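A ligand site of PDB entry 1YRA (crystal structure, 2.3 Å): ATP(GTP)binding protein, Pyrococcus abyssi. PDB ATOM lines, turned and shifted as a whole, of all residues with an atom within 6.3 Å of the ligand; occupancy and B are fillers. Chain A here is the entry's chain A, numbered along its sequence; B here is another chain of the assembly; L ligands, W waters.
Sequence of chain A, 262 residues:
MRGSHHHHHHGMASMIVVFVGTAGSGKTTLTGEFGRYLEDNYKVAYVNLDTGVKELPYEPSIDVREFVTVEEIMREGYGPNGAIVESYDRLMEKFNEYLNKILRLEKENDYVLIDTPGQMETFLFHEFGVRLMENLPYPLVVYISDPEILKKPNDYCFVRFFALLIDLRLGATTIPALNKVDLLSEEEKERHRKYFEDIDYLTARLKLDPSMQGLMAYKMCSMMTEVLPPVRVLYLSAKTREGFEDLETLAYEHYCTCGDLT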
ATOM      1  N   GLY A  21      18.486   0.855 -18.447  1.00  0.00           N
ATOM      2  CA  GLY A  21      19.669   0.340 -17.771  1.00  0.00           C
ATOM      3  C   GLY A  21      20.815   0.478 -18.742  1.00  0.00           C
ATOM      4  O   GLY A  21      20.613   0.549 -19.941  1.00  0.00           O
ATOM      5  N   THR A  22      22.041   0.566 -18.233  1.00  0.00           N
ATOM      6  CA  THR A  22      23.171   0.580 -19.139  1.00  0.00           C
ATOM      7  C   THR A  22      23.200  -0.709 -19.946  1.00  0.00           C
ATOM      8  O   THR A  22      22.661  -1.741 -19.521  1.00  0.00           O
ATOM      9  CB  THR A  22      24.492   0.733 -18.404  1.00  0.00           C
ATOM     10  OG1 THR A  22      25.524   0.971 -19.363  1.00  0.00           O
ATOM     11  CG2 THR A  22      24.840  -0.536 -17.594  1.00  0.00           C
ATOM     12  N   ALA A  23      23.804  -0.634 -21.135  1.00  0.00           N
ATOM     13  CA  ALA A  23      24.124  -1.822 -21.935  1.00  0.00           C
ATOM     14  C   ALA A  23      24.713  -2.944 -21.071  1.00  0.00           C
ATOM     15  O   ALA A  23      25.718  -2.739 -20.387  1.00  0.00           O
ATOM     16  CB  ALA A  23      25.095  -1.453 -23.049  1.00  0.00           C
ATOM     17  N   GLY A  24      24.052  -4.105 -21.088  1.00  0.00           N
ATOM     18  CA  GLY A  24      24.521  -5.287 -20.351  1.00  0.00           C
ATOM     19  C   GLY A  24      23.847  -5.557 -19.010  1.00  0.00           C
ATOM     20  O   GLY A  24      24.060  -6.615 -18.407  1.00  0.00           O
ATOM     21  N   SER A  25      23.035  -4.618 -18.528  1.00  0.00           N
ATOM     22  CA  SER A  25      22.368  -4.840 -17.242  1.00  0.00           C
ATOM     23  C   SER A  25      21.269  -5.888 -17.321  1.00  0.00           C
ATOM     24  O   SER A  25      20.839  -6.443 -16.285  1.00  0.00           O
ATOM     25  CB  SER A  25      21.827  -3.538 -16.661  1.00  0.00           C
ATOM     26  OG  SER A  25      21.234  -2.749 -17.658  1.00  0.00           O
ATOM     27  N   GLY A  26      20.793  -6.154 -18.540  1.00  0.00           N
ATOM     28  CA  GLY A  26      19.737  -7.144 -18.710  1.00  0.00           C
ATOM     29  C   GLY A  26      18.381  -6.610 -19.115  1.00  0.00           C
ATOM     30  O   GLY A  26      17.372  -7.226 -18.786  1.00  0.00           O
ATOM     31  N   LYS A  27      18.350  -5.512 -19.858  1.00  0.00           N
ATOM     32  CA  LYS A  27      17.077  -4.894 -20.290  1.00  0.00           C
ATOM     33  C   LYS A  27      16.212  -5.843 -21.118  1.00  0.00           C
ATOM     34  O   LYS A  27      15.034  -6.061 -20.799  1.00  0.00           O
ATOM     35  CB  LYS A  27      17.326  -3.623 -21.100  1.00  0.00           C
ATOM     36  CG  LYS A  27      17.608  -2.380 -20.271  1.00  0.00           C
ATOM     37  CD  LYS A  27      17.842  -1.168 -21.176  1.00  0.00           C
ATOM     38  CE  LYS A  27      18.891  -1.473 -22.237  1.00  0.00           C
ATOM     39  NZ  LYS A  27      20.301  -1.714 -21.701  1.00  0.00           N
ATOM     40  N   THR A  28      16.808  -6.400 -22.162  1.00  0.00           N
ATOM     41  CA  THR A  28      16.122  -7.246 -23.123  1.00  0.00           C
ATOM     42  C   THR A  28      15.679  -8.555 -22.490  1.00  0.00           C
ATOM     43  O   THR A  28      14.576  -9.035 -22.759  1.00  0.00           O
ATOM     44  CB  THR A  28      17.025  -7.432 -24.370  1.00  0.00           C
ATOM     45  OG1 THR A  28      17.013  -6.214 -25.127  1.00  0.00           O
ATOM     46  CG2 THR A  28      16.549  -8.545 -25.279  1.00  0.00           C
ATOM     47  N   THR A  29      16.493  -9.087 -21.587  1.00  0.00           N
ATOM     48  CA  THR A  29      16.162 -10.337 -20.902  1.00  0.00           C
ATOM     49  C   THR A  29      15.010 -10.116 -19.949  1.00  0.00           C
ATOM     50  O   THR A  29      14.063 -10.901 -19.933  1.00  0.00           O
ATOM     51  CB  THR A  29      17.374 -10.895 -20.085  1.00  0.00           C
ATOM     52  OG1 THR A  29      18.473 -11.084 -20.960  1.00  0.00           O
ATOM     53  CG2 THR A  29      17.035 -12.254 -19.462  1.00  0.00           C
ATOM     54  N   LEU A  30      15.098  -9.066 -19.148  1.00  0.00           N
ATOM     55  CA  LEU A  30      14.004  -8.721 -18.253  1.00  0.00           C
ATOM     56  C   LEU A  30      12.648  -8.479 -18.949  1.00  0.00           C
ATOM     57  O   LEU A  30      11.599  -8.902 -18.451  1.00  0.00           O
ATOM     58  CB  LEU A  30      14.415  -7.520 -17.401  1.00  0.00           C
ATOM     59  CG  LEU A  30      13.425  -7.027 -16.356  1.00  0.00           C
ATOM     60  CD1 LEU A  30      12.940  -8.197 -15.471  1.00  0.00           C
ATOM     61  CD2 LEU A  30      14.123  -5.955 -15.504  1.00  0.00           C
ATOM     62  N   ASP A  50      15.294  -0.654 -29.678  1.00  0.00           N
ATOM     63  CA  ASP A  50      16.731  -0.844 -29.786  1.00  0.00           C
ATOM     64  C   ASP A  50      17.075  -1.318 -31.178  1.00  0.00           C
ATOM     65  O   ASP A  50      16.686  -2.409 -31.594  1.00  0.00           O
ATOM     66  CB  ASP A  50      17.166  -1.859 -28.716  1.00  0.00           C
ATOM     67  CG  ASP A  50      18.679  -2.149 -28.710  1.00  0.00           C
ATOM     68  OD1 ASP A  50      19.490  -1.539 -29.465  1.00  0.00           O
ATOM     69  OD2 ASP A  50      19.052  -3.036 -27.914  1.00  0.00           O
ATOM     70  N   VAL A  53      20.355  -4.493 -31.013  1.00  0.00           N
ATOM     71  CA  VAL A  53      20.204  -5.871 -30.564  1.00  0.00           C
ATOM     72  C   VAL A  53      20.190  -6.884 -31.726  1.00  0.00           C
ATOM     73  O   VAL A  53      19.587  -6.642 -32.779  1.00  0.00           O
ATOM     74  CB  VAL A  53      18.936  -6.015 -29.730  1.00  0.00           C
ATOM     75  CG1 VAL A  53      17.710  -5.666 -30.559  1.00  0.00           C
ATOM     76  CG2 VAL A  53      18.824  -7.430 -29.130  1.00  0.00           C
ATOM     77  N   ASP A 115      11.228  -1.951 -24.333  1.00  0.00           N
ATOM     78  CA  ASP A 115      12.618  -2.331 -24.240  1.00  0.00           C
ATOM     79  C   ASP A 115      13.357  -1.226 -24.992  1.00  0.00           C
ATOM     80  O   ASP A 115      13.204  -1.071 -26.202  1.00  0.00           O
ATOM     81  CB  ASP A 115      12.821  -3.695 -24.921  1.00  0.00           C
ATOM     82  CG  ASP A 115      14.201  -4.291 -24.665  1.00  0.00           C
ATOM     83  OD1 ASP A 115      14.919  -3.836 -23.734  1.00  0.00           O
ATOM     84  OD2 ASP A 115      14.581  -5.215 -25.435  1.00  0.00           O
ATOM     85  N   GLY A 118      19.793   0.092 -26.441  1.00  0.00           N
ATOM     86  CA  GLY A 118      20.695  -0.769 -25.671  1.00  0.00           C
ATOM     87  C   GLY A 118      21.610   0.084 -24.820  1.00  0.00           C
ATOM     88  O   GLY A 118      22.029  -0.313 -23.734  1.00  0.00           O
ATOM     89  N   ILE A 144      17.272  -0.410 -14.033  1.00  0.00           N
ATOM     90  CA  ILE A 144      18.010  -1.546 -13.472  1.00  0.00           C
ATOM     91  C   ILE A 144      19.509  -1.372 -13.505  1.00  0.00           C
ATOM     92  O   ILE A 144      20.084  -0.788 -14.439  1.00  0.00           O
ATOM     93  CB  ILE A 144      17.701  -2.889 -14.180  1.00  0.00           C
ATOM     94  CG1 ILE A 144      18.107  -2.828 -15.658  1.00  0.00           C
ATOM     95  CG2 ILE A 144      16.269  -3.266 -14.029  1.00  0.00           C
ATOM     96  CD1 ILE A 144      17.676  -4.045 -16.444  1.00  0.00           C
ATOM     97  N   ASN A 179      19.262  -5.952 -11.062  1.00  0.00           N
ATOM     98  CA  ASN A 179      19.050  -7.170 -11.823  1.00  0.00           C
ATOM     99  C   ASN A 179      20.143  -8.159 -11.492  1.00  0.00           C
ATOM    100  O   ASN A 179      21.101  -7.808 -10.790  1.00  0.00           O
ATOM    101  CB  ASN A 179      19.042  -6.907 -13.332  1.00  0.00           C
ATOM    102  CG  ASN A 179      18.420  -8.059 -14.132  1.00  0.00           C
ATOM    103  OD1 ASN A 179      18.876  -8.374 -15.224  1.00  0.00           O
ATOM    104  ND2 ASN A 179      17.388  -8.679 -13.587  1.00  0.00           N
ATOM    105  N   LYS A 180      20.012  -9.392 -11.988  1.00  0.00           N
ATOM    106  CA  LYS A 180      21.012 -10.421 -11.767  1.00  0.00           C
ATOM    107  C   LYS A 180      21.195 -10.730 -10.272  1.00  0.00           C
ATOM    108  O   LYS A 180      22.291 -11.132  -9.840  1.00  0.00           O
ATOM    109  CB  LYS A 180      22.340 -10.020 -12.434  1.00  0.00           C
ATOM    110  CG  LYS A 180      22.190  -9.482 -13.844  1.00  0.00           C
ATOM    111  CD  LYS A 180      23.533  -9.318 -14.582  1.00  0.00           C
ATOM    112  CE  LYS A 180      23.387  -8.348 -15.743  1.00  0.00           C
ATOM    113  NZ  LYS A 180      24.417  -8.494 -16.838  1.00  0.00           N
ATOM    114  N   VAL A 181      20.140 -10.571  -9.479  1.00  0.00           N
ATOM    115  CA  VAL A 181      20.235 -10.903  -8.067  1.00  0.00           C
ATOM    116  C   VAL A 181      20.441 -12.400  -7.818  1.00  0.00           C
ATOM    117  O   VAL A 181      20.871 -12.810  -6.733  1.00  0.00           O
ATOM    118  CB  VAL A 181      19.051 -10.396  -7.209  1.00  0.00           C
ATOM    119  CG1 VAL A 181      18.967  -8.852  -7.202  1.00  0.00           C
ATOM    120  CG2 VAL A 181      17.767 -11.013  -7.659  1.00  0.00           C
ATOM    121  N   ASP A 182      20.137 -13.213  -8.833  1.00  0.00           N
ATOM    122  CA  ASP A 182      20.414 -14.647  -8.794  1.00  0.00           C
ATOM    123  C   ASP A 182      21.863 -14.944  -8.433  1.00  0.00           C
ATOM    124  O   ASP A 182      22.151 -15.910  -7.733  1.00  0.00           O
ATOM    125  CB  ASP A 182      20.013 -15.351 -10.113  1.00  0.00           C
ATOM    126  CG  ASP A 182      20.511 -14.642 -11.346  1.00  0.00           C
ATOM    127  OD1 ASP A 182      20.098 -13.483 -11.591  1.00  0.00           O
ATOM    128  OD2 ASP A 182      21.307 -15.226 -12.111  1.00  0.00           O
ATOM    129  N   LEU A 183      22.775 -14.095  -8.893  1.00  0.00           N
ATOM    130  CA  LEU A 183      24.212 -14.284  -8.664  1.00  0.00           C
ATOM    131  C   LEU A 183      24.718 -13.851  -7.271  1.00  0.00           C
ATOM    132  O   LEU A 183      25.874 -14.073  -6.923  1.00  0.00           O
ATOM    133  CB  LEU A 183      25.013 -13.526  -9.710  1.00  0.00           C
ATOM    134  CG  LEU A 183      24.706 -13.720 -11.188  1.00  0.00           C
ATOM    135  CD1 LEU A 183      25.476 -12.689 -11.995  1.00  0.00           C
ATOM    136  CD2 LEU A 183      25.077 -15.126 -11.633  1.00  0.00           C
ATOM    137  N   LEU A 236      15.606  -7.817  -8.591  1.00  0.00           N
ATOM    138  CA  LEU A 236      15.023  -8.648  -9.629  1.00  0.00           C
ATOM    139  C   LEU A 236      15.994  -9.651 -10.152  1.00  0.00           C
ATOM    140  O   LEU A 236      17.219  -9.448 -10.117  1.00  0.00           O
ATOM    141  CB  LEU A 236      14.539  -7.791 -10.821  1.00  0.00           C
ATOM    142  CG  LEU A 236      13.494  -6.718 -10.548  1.00  0.00           C
ATOM    143  CD1 LEU A 236      13.388  -5.743 -11.717  1.00  0.00           C
ATOM    144  CD2 LEU A 236      12.141  -7.353 -10.216  1.00  0.00           C
ATOM    145  N   SER A 237      15.438 -10.744 -10.666  1.00  0.00           N
ATOM    146  CA  SER A 237      16.211 -11.632 -11.501  1.00  0.00           C
ATOM    147  C   SER A 237      15.440 -11.998 -12.764  1.00  0.00           C
ATOM    148  O   SER A 237      14.391 -12.626 -12.700  1.00  0.00           O
ATOM    149  CB  SER A 237      16.608 -12.893 -10.748  1.00  0.00           C
ATOM    150  OG  SER A 237      17.508 -13.596 -11.575  1.00  0.00           O
ATOM    151  N   ALA A 238      15.991 -11.595 -13.911  1.00  0.00           N
ATOM    152  CA  ALA A 238      15.384 -11.859 -15.200  1.00  0.00           C
ATOM    153  C   ALA A 238      15.586 -13.314 -15.594  1.00  0.00           C
ATOM    154  O   ALA A 238      14.985 -13.791 -16.564  1.00  0.00           O
ATOM    155  CB  ALA A 238      15.972 -10.929 -16.262  1.00  0.00           C
ATOM    156  N   LYS A 239      16.417 -14.016 -14.843  1.00  0.00           N
ATOM    157  CA  LYS A 239      16.656 -15.436 -15.085  1.00  0.00           C
ATOM    158  C   LYS A 239      15.672 -16.288 -14.284  1.00  0.00           C
ATOM    159  O   LYS A 239      15.105 -17.249 -14.814  1.00  0.00           O
ATOM    160  CB  LYS A 239      18.109 -15.793 -14.743  1.00  0.00           C
ATOM    161  CG  LYS A 239      18.603 -17.144 -15.276  1.00  0.00           C
ATOM    162  CD  LYS A 239      20.141 -17.156 -15.409  1.00  0.00           C
ATOM    163  CE  LYS A 239      20.726 -18.582 -15.264  1.00  0.00           C
ATOM    164  NZ  LYS A 239      20.870 -18.988 -13.833  1.00  0.00           N
ATOM    165  N   THR A 240      15.421 -15.918 -13.025  1.00  0.00           N
ATOM    166  CA  THR A 240      14.613 -16.746 -12.128  1.00  0.00           C
ATOM    167  C   THR A 240      13.253 -16.176 -11.713  1.00  0.00           C
ATOM    168  O   THR A 240      12.482 -16.845 -11.009  1.00  0.00           O
ATOM    169  CB  THR A 240      15.348 -17.017 -10.806  1.00  0.00           C
ATOM    170  OG1 THR A 240      15.223 -15.867  -9.948  1.00  0.00           O
ATOM    171  CG2 THR A 240      16.818 -17.321 -11.050  1.00  0.00           C
ATOM    172  N   ASN B  81      26.138  -3.349 -29.290  1.00  0.00           N
ATOM    173  CA  ASN B  81      26.129  -3.020 -27.880  1.00  0.00           C
ATOM    174  C   ASN B  81      26.683  -4.167 -27.042  1.00  0.00           C
ATOM    175  O   ASN B  81      27.373  -3.933 -26.032  1.00  0.00           O
ATOM    176  CB  ASN B  81      24.697  -2.662 -27.435  1.00  0.00           C
ATOM    177  CG  ASN B  81      24.158  -1.455 -28.177  1.00  0.00           C
ATOM    178  OD1 ASN B  81      24.810  -0.412 -28.217  1.00  0.00           O
ATOM    179  ND2 ASN B  81      22.985  -1.598 -28.822  1.00  0.00           N
HETATM  180  P1  LIG L   1      20.793  -5.369 -22.230  1.00  0.00           P
HETATM  181  O1  LIG L   1      19.639  -5.596 -23.190  1.00  0.00           O
HETATM  182  O2  LIG L   1      21.995  -4.840 -22.952  1.00  0.00           O
HETATM  183  O3  LIG L   1      20.408  -4.296 -21.246  1.00  0.00           O
HETATM  184  O4  LIG L   1      21.090  -6.692 -21.344  1.00  0.00           O
HETATM  185  P2  LIG L   1      20.859  -8.200 -21.872  1.00  0.00           P
HETATM  186  O5  LIG L   1      19.441  -8.652 -21.670  1.00  0.00           O
HETATM  187  O6  LIG L   1      21.336  -8.224 -23.270  1.00  0.00           O
HETATM  188  O7  LIG L   1      21.709  -9.154 -20.881  1.00  0.00           O
HETATM  189  C1  LIG L   1      23.133  -9.056 -20.744  1.00  0.00           C
HETATM  190  C2  LIG L   1      23.653 -10.429 -20.319  1.00  0.00           C
HETATM  191  O8  LIG L   1      23.297 -10.637 -18.954  1.00  0.00           O
HETATM  192  C3  LIG L   1      23.017 -11.579 -21.099  1.00  0.00           C
HETATM  193  O9  LIG L   1      23.991 -12.605 -21.305  1.00  0.00           O
HETATM  194  C4  LIG L   1      21.958 -12.113 -20.181  1.00  0.00           C
HETATM  195  O10 LIG L   1      21.736 -13.505 -20.396  1.00  0.00           O
HETATM  196  C5  LIG L   1      22.530 -11.834 -18.798  1.00  0.00           C
HETATM  197  N1  LIG L   1      21.481 -11.545 -17.799  1.00  0.00           N
HETATM  198  C6  LIG L   1      20.506 -10.634 -17.903  1.00  0.00           C
HETATM  199  N2  LIG L   1      19.728 -10.632 -16.782  1.00  0.00           N
HETATM  200  C7  LIG L   1      20.208 -11.565 -15.951  1.00  0.00           C
HETATM  201  C8  LIG L   1      19.863 -12.055 -14.617  1.00  0.00           C
HETATM  202  O11 LIG L   1      18.878 -11.565 -14.004  1.00  0.00           O
HETATM  203  N3  LIG L   1      20.633 -13.030 -14.097  1.00  0.00           N
HETATM  204  C9  LIG L   1      21.696 -13.564 -14.752  1.00  0.00           C
HETATM  205  N4  LIG L   1      22.429 -14.565 -14.184  1.00  0.00           N
HETATM  206  N5  LIG L   1      22.056 -13.139 -15.981  1.00  0.00           N
HETATM  207  C10 LIG L   1      21.373 -12.158 -16.612  1.00  0.00           C
HETATM  208  O   HOH W   1      20.215 -15.195 -18.419  1.00  0.00           O
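An oxygen (O2) of the ligand is in hydrogen-bond range of the backbone NH (N) of Gly 24, at 2.9 Å. N of Thr 29 lies within hydrogen-bond range of O5 of the ligand. The side-chain hydroxyl (OG1) of Thr 29 lies within hydrogen-bond range of an oxygen (O5) of the ligand. OD1 of Asn 179 sits close to N2 of the ligand (2.9 Å). N of Lys 180 sits at hydrogen-bond distance from O11 of the ligand (3.2 Å). OG of Ser 237 lies within hydrogen-bond range of O11 of the ligand (3.4 Å). NZ of Lys 27 is in salt-bridge range of O3 of the ligand, 2.6 Å away. An oxygen (O1) of the ligand is in hydrogen-bond range of the side-chain hydroxyl of Thr 28, 3.3 Å away. The backbone NH (N) of Lys 27 lies within hydrogen-bond range of an oxygen (O3) of the ligand, at 2.8 Å. An oxygen (O11) of the ligand lies within hydrogen-bond range of the backbone NH of Ala 238, at 2.9 Å. The side-chain carboxylate (OD2) of Asp 182 lies within hydrogen-bond range of a nitrogen (N4) of the ligand, 2.4 Å away. The backbone NH of Thr 28 is in hydrogen-bond range of an oxygen (O1) of the ligand, at 3.1 Å. The backbone NH (N) of Gly 26 is in hydrogen-bond range of an oxygen (O4) of the ligand, at 2.9 Å. An oxygen (O8) of the ligand lies within hydrogen-bond range of the side-chain amino group of Lys 180, 3.2 Å away.
Thr 22 touches the ligand. Ala 23 touches the ligand. N of Ser 25 touches O3 of the ligand, 3.8 Å away. Leu 183 touches the ligand (CD2 to N4, 3.7 Å). N of Lys 239 touches O11 of the ligand, at 3.6 Å. Within 4 Å of the ligand: Thr 22, Ala 23, Gly 24, Ser 25, Gly 26, Lys 27, Thr 28, Thr 29, Asn 179, Lys 180, Asp 182, Leu 183, Ser 237, Ala 238 and Lys 239. The nearest printed residue that does not touch the ligand is Gly 118 (4.6 Å).
N of Lys 239 sits close to OG of Ser 237 (3.5 Å). The side-chain amide oxygen (OD1) of Asn 179 sits close to the backbone carbonyl oxygen (O) of Ser 25 (3.0 Å). The backbone carbonyl oxygen of Gly 118 sits close to the backbone NH of Ala 23, 3.2 Å away. O of Gly 118 is in hydrogen-bond range of NZ of Lys 27 (3.0 Å). The side-chain hydroxyl of Thr 28 lies within hydrogen-bond range of the side-chain carboxylate of Asp 115. The side-chain amide nitrogen (ND2) of Asn 179 sits close to the backbone NH (N) of Ala 238 (3.2 Å). The side-chain hydroxyl (OG) of Ser 237 sits at hydrogen-bond distance from the backbone NH (N) of Thr 240, at 3.4 Å. O of Thr 22 lies within hydrogen-bond range of NZ of Lys 27 (3.2 Å).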
